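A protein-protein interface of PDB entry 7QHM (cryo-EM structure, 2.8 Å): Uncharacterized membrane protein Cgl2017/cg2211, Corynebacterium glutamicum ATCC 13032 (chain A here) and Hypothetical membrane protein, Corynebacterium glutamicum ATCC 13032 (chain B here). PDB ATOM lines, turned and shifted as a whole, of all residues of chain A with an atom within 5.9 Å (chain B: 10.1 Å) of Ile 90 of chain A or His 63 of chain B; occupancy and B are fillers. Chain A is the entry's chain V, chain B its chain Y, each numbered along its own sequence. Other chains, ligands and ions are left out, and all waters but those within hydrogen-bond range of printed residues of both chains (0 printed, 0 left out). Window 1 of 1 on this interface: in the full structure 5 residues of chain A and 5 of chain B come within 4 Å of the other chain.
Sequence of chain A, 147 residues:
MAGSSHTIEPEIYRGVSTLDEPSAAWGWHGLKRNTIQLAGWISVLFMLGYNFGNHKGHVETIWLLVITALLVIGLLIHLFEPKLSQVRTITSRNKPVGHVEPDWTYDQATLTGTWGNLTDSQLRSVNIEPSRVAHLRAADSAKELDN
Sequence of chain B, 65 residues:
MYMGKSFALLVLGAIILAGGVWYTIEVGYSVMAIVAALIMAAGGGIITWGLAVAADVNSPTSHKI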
ATOM      1  N   ARG A  88     -11.822 -20.467 -15.023  1.00  0.00           N
ATOM      2  CA  ARG A  88     -11.873 -19.036 -15.299  1.00  0.00           C
ATOM      3  C   ARG A  88     -12.815 -18.376 -14.301  1.00  0.00           C
ATOM      4  O   ARG A  88     -13.904 -17.918 -14.643  1.00  0.00           O
ATOM      5  CB  ARG A  88     -12.326 -18.792 -16.739  1.00  0.00           C
ATOM      6  CG  ARG A  88     -11.579 -19.589 -17.793  1.00  0.00           C
ATOM      7  CD  ARG A  88     -10.107 -19.237 -17.849  1.00  0.00           C
ATOM      8  NE  ARG A  88      -9.388 -20.076 -18.799  1.00  0.00           N
ATOM      9  CZ  ARG A  88      -8.147 -19.858 -19.217  1.00  0.00           C
ATOM     10  NH1 ARG A  88      -7.448 -18.811 -18.804  1.00  0.00           N
ATOM     11  NH2 ARG A  88      -7.593 -20.710 -20.074  1.00  0.00           N
ATOM     12  N   THR A  89     -12.383 -18.352 -13.047  1.00  0.00           N
ATOM     13  CA  THR A  89     -13.127 -17.752 -11.956  1.00  0.00           C
ATOM     14  C   THR A  89     -12.211 -16.800 -11.210  1.00  0.00           C
ATOM     15  O   THR A  89     -11.009 -16.732 -11.466  1.00  0.00           O
ATOM     16  CB  THR A  89     -13.680 -18.807 -10.984  1.00  0.00           C
ATOM     17  OG1 THR A  89     -12.605 -19.565 -10.426  1.00  0.00           O
ATOM     18  CG2 THR A  89     -14.634 -19.750 -11.685  1.00  0.00           C
ATOM     19  N   ILE A  90     -12.798 -16.051 -10.286  1.00  0.00           N
ATOM     20  CA  ILE A  90     -12.047 -15.227  -9.355  1.00  0.00           C
ATOM     21  C   ILE A  90     -12.614 -15.465  -7.969  1.00  0.00           C
ATOM     22  O   ILE A  90     -13.809 -15.264  -7.735  1.00  0.00           O
ATOM     23  CB  ILE A  90     -12.080 -13.738  -9.738  1.00  0.00           C
ATOM     24  CG1 ILE A  90     -11.013 -13.449 -10.805  1.00  0.00           C
ATOM     25  CG2 ILE A  90     -11.875 -12.826  -8.526  1.00  0.00           C
ATOM     26  CD1 ILE A  90      -9.544 -13.542 -10.325  1.00  0.00           C
ATOM     27  N   THR A  91     -11.746 -15.886  -7.058  1.00  0.00           N
ATOM     28  CA  THR A  91     -12.110 -16.346  -5.733  1.00  0.00           C
ATOM     29  C   THR A  91     -11.470 -15.417  -4.719  1.00  0.00           C
ATOM     30  O   THR A  91     -10.272 -15.139  -4.808  1.00  0.00           O
ATOM     31  CB  THR A  91     -11.628 -17.783  -5.520  1.00  0.00           C
ATOM     32  OG1 THR A  91     -12.298 -18.650  -6.438  1.00  0.00           O
ATOM     33  CG2 THR A  91     -11.888 -18.259  -4.111  1.00  0.00           C
ATOM     34  N   SER A  92     -12.266 -14.942  -3.771  1.00  0.00           N
ATOM     35  CA  SER A  92     -11.755 -14.177  -2.630  1.00  0.00           C
ATOM     36  C   SER A  92     -11.087 -12.914  -3.177  1.00  0.00           C
ATOM     37  O   SER A  92     -11.562 -12.351  -4.175  1.00  0.00           O
ATOM     38  CB  SER A  92     -10.864 -15.066  -1.800  1.00  0.00           C
ATOM     39  OG  SER A  92     -10.481 -14.421  -0.603  1.00  0.00           O
ATOM     40  N   ASN A  94      -8.383 -12.585  -4.840  1.00  0.00           N
ATOM     41  CA  ASN A  94      -7.544 -12.789  -6.007  1.00  0.00           C
ATOM     42  C   ASN A  94      -8.020 -11.870  -7.121  1.00  0.00           C
ATOM     43  O   ASN A  94      -9.211 -11.579  -7.240  1.00  0.00           O
ATOM     44  CB  ASN A  94      -7.604 -14.254  -6.456  1.00  0.00           C
ATOM     45  CG  ASN A  94      -6.455 -14.645  -7.360  1.00  0.00           C
ATOM     46  OD1 ASN A  94      -5.420 -13.995  -7.382  1.00  0.00           O
ATOM     47  ND2 ASN A  94      -6.635 -15.718  -8.106  1.00  0.00           N
ATOM     48  N   LYS A  95      -7.080 -11.410  -7.932  1.00  0.00           N
ATOM     49  CA  LYS A  95      -7.333 -10.455  -8.995  1.00  0.00           C
ATOM     50  C   LYS A  95      -7.250 -11.148 -10.350  1.00  0.00           C
ATOM     51  O   LYS A  95      -6.621 -12.203 -10.470  1.00  0.00           O
ATOM     52  CB  LYS A  95      -6.313  -9.311  -8.945  1.00  0.00           C
ATOM     53  CG  LYS A  95      -6.232  -8.574  -7.618  1.00  0.00           C
ATOM     54  CD  LYS A  95      -7.464  -7.739  -7.362  1.00  0.00           C
ATOM     55  CE  LYS A  95      -7.348  -6.989  -6.050  1.00  0.00           C
ATOM     56  NZ  LYS A  95      -8.464  -6.025  -5.862  1.00  0.00           N
ATOM     57  N   PRO A  96      -7.876 -10.594 -11.393  1.00  0.00           N
ATOM     58  CA  PRO A  96      -7.795 -11.225 -12.716  1.00  0.00           C
ATOM     59  C   PRO A  96      -6.371 -11.335 -13.234  1.00  0.00           C
ATOM     60  O   PRO A  96      -5.456 -10.645 -12.789  1.00  0.00           O
ATOM     61  CB  PRO A  96      -8.634 -10.300 -13.597  1.00  0.00           C
ATOM     62  CG  PRO A  96      -9.600  -9.719 -12.683  1.00  0.00           C
ATOM     63  CD  PRO A  96      -8.855  -9.495 -11.406  1.00  0.00           C
ATOM     64  N   VAL A  97      -6.200 -12.236 -14.198  1.00  0.00           N
ATOM     65  CA  VAL A  97      -4.889 -12.459 -14.785  1.00  0.00           C
ATOM     66  C   VAL A  97      -4.431 -11.197 -15.506  1.00  0.00           C
ATOM     67  O   VAL A  97      -5.239 -10.404 -16.003  1.00  0.00           O
ATOM     68  CB  VAL A  97      -4.938 -13.667 -15.737  1.00  0.00           C
ATOM     69  CG1 VAL A  97      -3.598 -13.885 -16.414  1.00  0.00           C
ATOM     70  CG2 VAL A  97      -5.360 -14.924 -14.975  1.00  0.00           C
ATOM     71  N   ASP B  56     -23.932 -23.251  -1.477  1.00  0.00           N
ATOM     72  CA  ASP B  56     -22.949 -22.461  -2.205  1.00  0.00           C
ATOM     73  C   ASP B  56     -23.590 -21.270  -2.899  1.00  0.00           C
ATOM     74  O   ASP B  56     -23.038 -20.166  -2.869  1.00  0.00           O
ATOM     75  CB  ASP B  56     -22.226 -23.322  -3.232  1.00  0.00           C
ATOM     76  CG  ASP B  56     -21.153 -22.555  -3.960  1.00  0.00           C
ATOM     77  OD1 ASP B  56     -20.148 -22.185  -3.317  1.00  0.00           O
ATOM     78  OD2 ASP B  56     -21.313 -22.308  -5.171  1.00  0.00           O
ATOM     79  N   VAL B  57     -24.747 -21.467  -3.537  1.00  0.00           N
ATOM     80  CA  VAL B  57     -25.387 -20.377  -4.272  1.00  0.00           C
ATOM     81  C   VAL B  57     -26.175 -19.452  -3.363  1.00  0.00           C
ATOM     82  O   VAL B  57     -26.753 -18.473  -3.846  1.00  0.00           O
ATOM     83  CB  VAL B  57     -26.291 -20.904  -5.405  1.00  0.00           C
ATOM     84  CG1 VAL B  57     -25.485 -21.778  -6.352  1.00  0.00           C
ATOM     85  CG2 VAL B  57     -27.492 -21.666  -4.870  1.00  0.00           C
ATOM     86  N   SER B  59     -24.513 -17.824  -1.005  1.00  0.00           N
ATOM     87  CA  SER B  59     -23.506 -16.774  -0.840  1.00  0.00           C
ATOM     88  C   SER B  59     -22.220 -17.215  -1.518  1.00  0.00           C
ATOM     89  O   SER B  59     -21.257 -17.627  -0.857  1.00  0.00           O
ATOM     90  CB  SER B  59     -23.270 -16.472   0.640  1.00  0.00           C
ATOM     91  OG  SER B  59     -22.489 -15.300   0.804  1.00  0.00           O
ATOM     92  N   PRO B  60     -22.164 -17.152  -2.850  1.00  0.00           N
ATOM     93  CA  PRO B  60     -20.976 -17.646  -3.554  1.00  0.00           C
ATOM     94  C   PRO B  60     -19.720 -16.882  -3.169  1.00  0.00           C
ATOM     95  O   PRO B  60     -19.743 -15.667  -2.964  1.00  0.00           O
ATOM     96  CB  PRO B  60     -21.318 -17.437  -5.032  1.00  0.00           C
ATOM     97  CG  PRO B  60     -22.782 -17.366  -5.083  1.00  0.00           C
ATOM     98  CD  PRO B  60     -23.214 -16.736  -3.799  1.00  0.00           C
ATOM     99  N   THR B  61     -18.619 -17.622  -3.060  1.00  0.00           N
ATOM    100  CA  THR B  61     -17.299 -17.058  -2.828  1.00  0.00           C
ATOM    101  C   THR B  61     -16.471 -16.992  -4.105  1.00  0.00           C
ATOM    102  O   THR B  61     -15.254 -16.796  -4.040  1.00  0.00           O
ATOM    103  CB  THR B  61     -16.573 -17.871  -1.758  1.00  0.00           C
ATOM    104  OG1 THR B  61     -16.718 -19.268  -2.042  1.00  0.00           O
ATOM    105  CG2 THR B  61     -17.148 -17.577  -0.389  1.00  0.00           C
ATOM    106  N   SER B  62     -17.106 -17.140  -5.264  1.00  0.00           N
ATOM    107  CA  SER B  62     -16.404 -17.096  -6.533  1.00  0.00           C
ATOM    108  C   SER B  62     -17.357 -16.606  -7.609  1.00  0.00           C
ATOM    109  O   SER B  62     -18.558 -16.876  -7.562  1.00  0.00           O
ATOM    110  CB  SER B  62     -15.844 -18.468  -6.909  1.00  0.00           C
ATOM    111  OG  SER B  62     -15.060 -18.995  -5.858  1.00  0.00           O
ATOM    112  N   HIS B  63     -16.806 -15.882  -8.575  1.00  0.00           N
ATOM    113  CA  HIS B  63     -17.532 -15.421  -9.746  1.00  0.00           C
ATOM    114  C   HIS B  63     -17.012 -16.126 -10.991  1.00  0.00           C
ATOM    115  O   HIS B  63     -15.848 -16.522 -11.061  1.00  0.00           O
ATOM    116  CB  HIS B  63     -17.402 -13.909  -9.907  1.00  0.00           C
ATOM    117  CG  HIS B  63     -18.225 -13.128  -8.933  1.00  0.00           C
ATOM    118  ND1 HIS B  63     -18.406 -11.766  -9.035  1.00  0.00           N
ATOM    119  CD2 HIS B  63     -18.917 -13.518  -7.837  1.00  0.00           C
ATOM    120  CE1 HIS B  63     -19.173 -11.350  -8.044  1.00  0.00           C
ATOM    121  NE2 HIS B  63     -19.496 -12.394  -7.302  1.00  0.00           N
ATOM    122  N   LYS B  64     -17.891 -16.280 -11.974  1.00  0.00           N
ATOM    123  CA  LYS B  64     -17.566 -16.995 -13.207  1.00  0.00           C
ATOM    124  C   LYS B  64     -16.916 -16.047 -14.220  1.00  0.00           C
ATOM    125  O   LYS B  64     -17.384 -15.877 -15.345  1.00  0.00           O
ATOM    126  CB  LYS B  64     -18.825 -17.640 -13.775  1.00  0.00           C
ATOM    127  CG  LYS B  64     -18.572 -18.793 -14.736  1.00  0.00           C
ATOM    128  CD  LYS B  64     -18.216 -20.080 -14.001  1.00  0.00           C
ATOM    129  CE  LYS B  64     -18.298 -21.285 -14.925  1.00  0.00           C
ATOM    130  NZ  LYS B  64     -18.043 -22.564 -14.207  1.00  0.00           N
ATOM    131  N   ILE B  65     -15.810 -15.437 -13.796  1.00  0.00           N
ATOM    132  CA  ILE B  65     -15.104 -14.439 -14.599  1.00  0.00           C
ATOM    133  C   ILE B  65     -13.651 -14.845 -14.809  1.00  0.00           C
ATOM    134  O   ILE B  65     -13.158 -14.846 -15.933  1.00  0.00           O
ATOM    135  CB  ILE B  65     -15.207 -13.032 -13.952  1.00  0.00           C
ATOM    136  CG1 ILE B  65     -14.617 -13.015 -12.530  1.00  0.00           C
ATOM    137  CG2 ILE B  65     -16.667 -12.585 -13.935  1.00  0.00           C
ATOM    138  CD1 ILE B  65     -14.636 -11.651 -11.854  1.00  0.00           C
ATOM    139  OXT ILE B  65     -12.932 -15.189 -13.879  1.00  0.00           O
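The chain-end carboxylate (OXT) of Ile 65 of chain B lies close to the backbone NH (N) of Thr 89 of chain A (3.3 Å).
OG1 of Thr 91 of chain A sits at hydrogen-bond distance from OG of Ser 62 of chain B.
N of His 63 of chain B lies within hydrogen-bond range of O of Ile 90 of chain A (3.2 Å).
The backbone carbonyl oxygen (O) of Arg 88 of chain A sits close to the backbone NH (N) of Ile 65 of chain B.
O of Arg 88 of chain A touches C of Lys 64 of chain B (3.6 Å).
Thr 89 of chain A touches His 63 of chain B.
CA of Ser 62 of chain B touches O of Ile 90 of chain A (3.4 Å).
Ile 90 of chain A touches Ile 65 of chain B (N to OXT, 3.7 Å).
O of Thr 61 of chain B touches CA of Thr 91 of chain A (3.6 Å).
Ser 92 of chain A touches Thr 61 of chain B.
Printed residues of chain B within 4 Å of Arg 88 of chain A: Lys 64 (3.6 Å) and Ile 65 (3.0 Å).
Thr 89 of chain A touches just these residues of chain B: His 63 and Ile 65.
Ile 90 of chain A touches just these residues of chain B: Ser 62, His 63 and Ile 65.
Of the printed residues of chain B, Ser 92 of chain A touches Thr 61 (3.5 Å).
No residue of chain B comes within 4 Å of Asn 94 of chain A.
No residue of chain B comes within 4 Å of Pro 96 of chain A.
Of the printed residues of chain A, Thr 61 of chain B touches Thr 91 (3.6 Å) and Ser 92 (3.5 Å).
Printed residues of chain A within 4 Å of Lys 64 of chain B: Arg 88.
The nearest residue of chain A that does not touch His 63 of chain B is Arg 88 of chain A (4.3 Å).
Of the 9 printed residues of chain B, 5 touch a printed residue of chain A.
Hydrophobic or aromatic side chains of chain B that line the printed part of chain A: Ile 65.
Of the 9 printed residues of chain A, 5 touch a printed residue of chain B.
Printed residues of chain A that touch a printed residue of chain B: Arg 88, Thr 89, Ile 90, Thr 91 and Ser 92.
Hydrophobic or aromatic side chains of chain A within 4 Å of the printed part of chain B: Ile 90.
Among the printed residues, no Asp or Glu carboxylate lies within 4 Å of a Lys or Arg side-chain nitrogen of the other chain.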
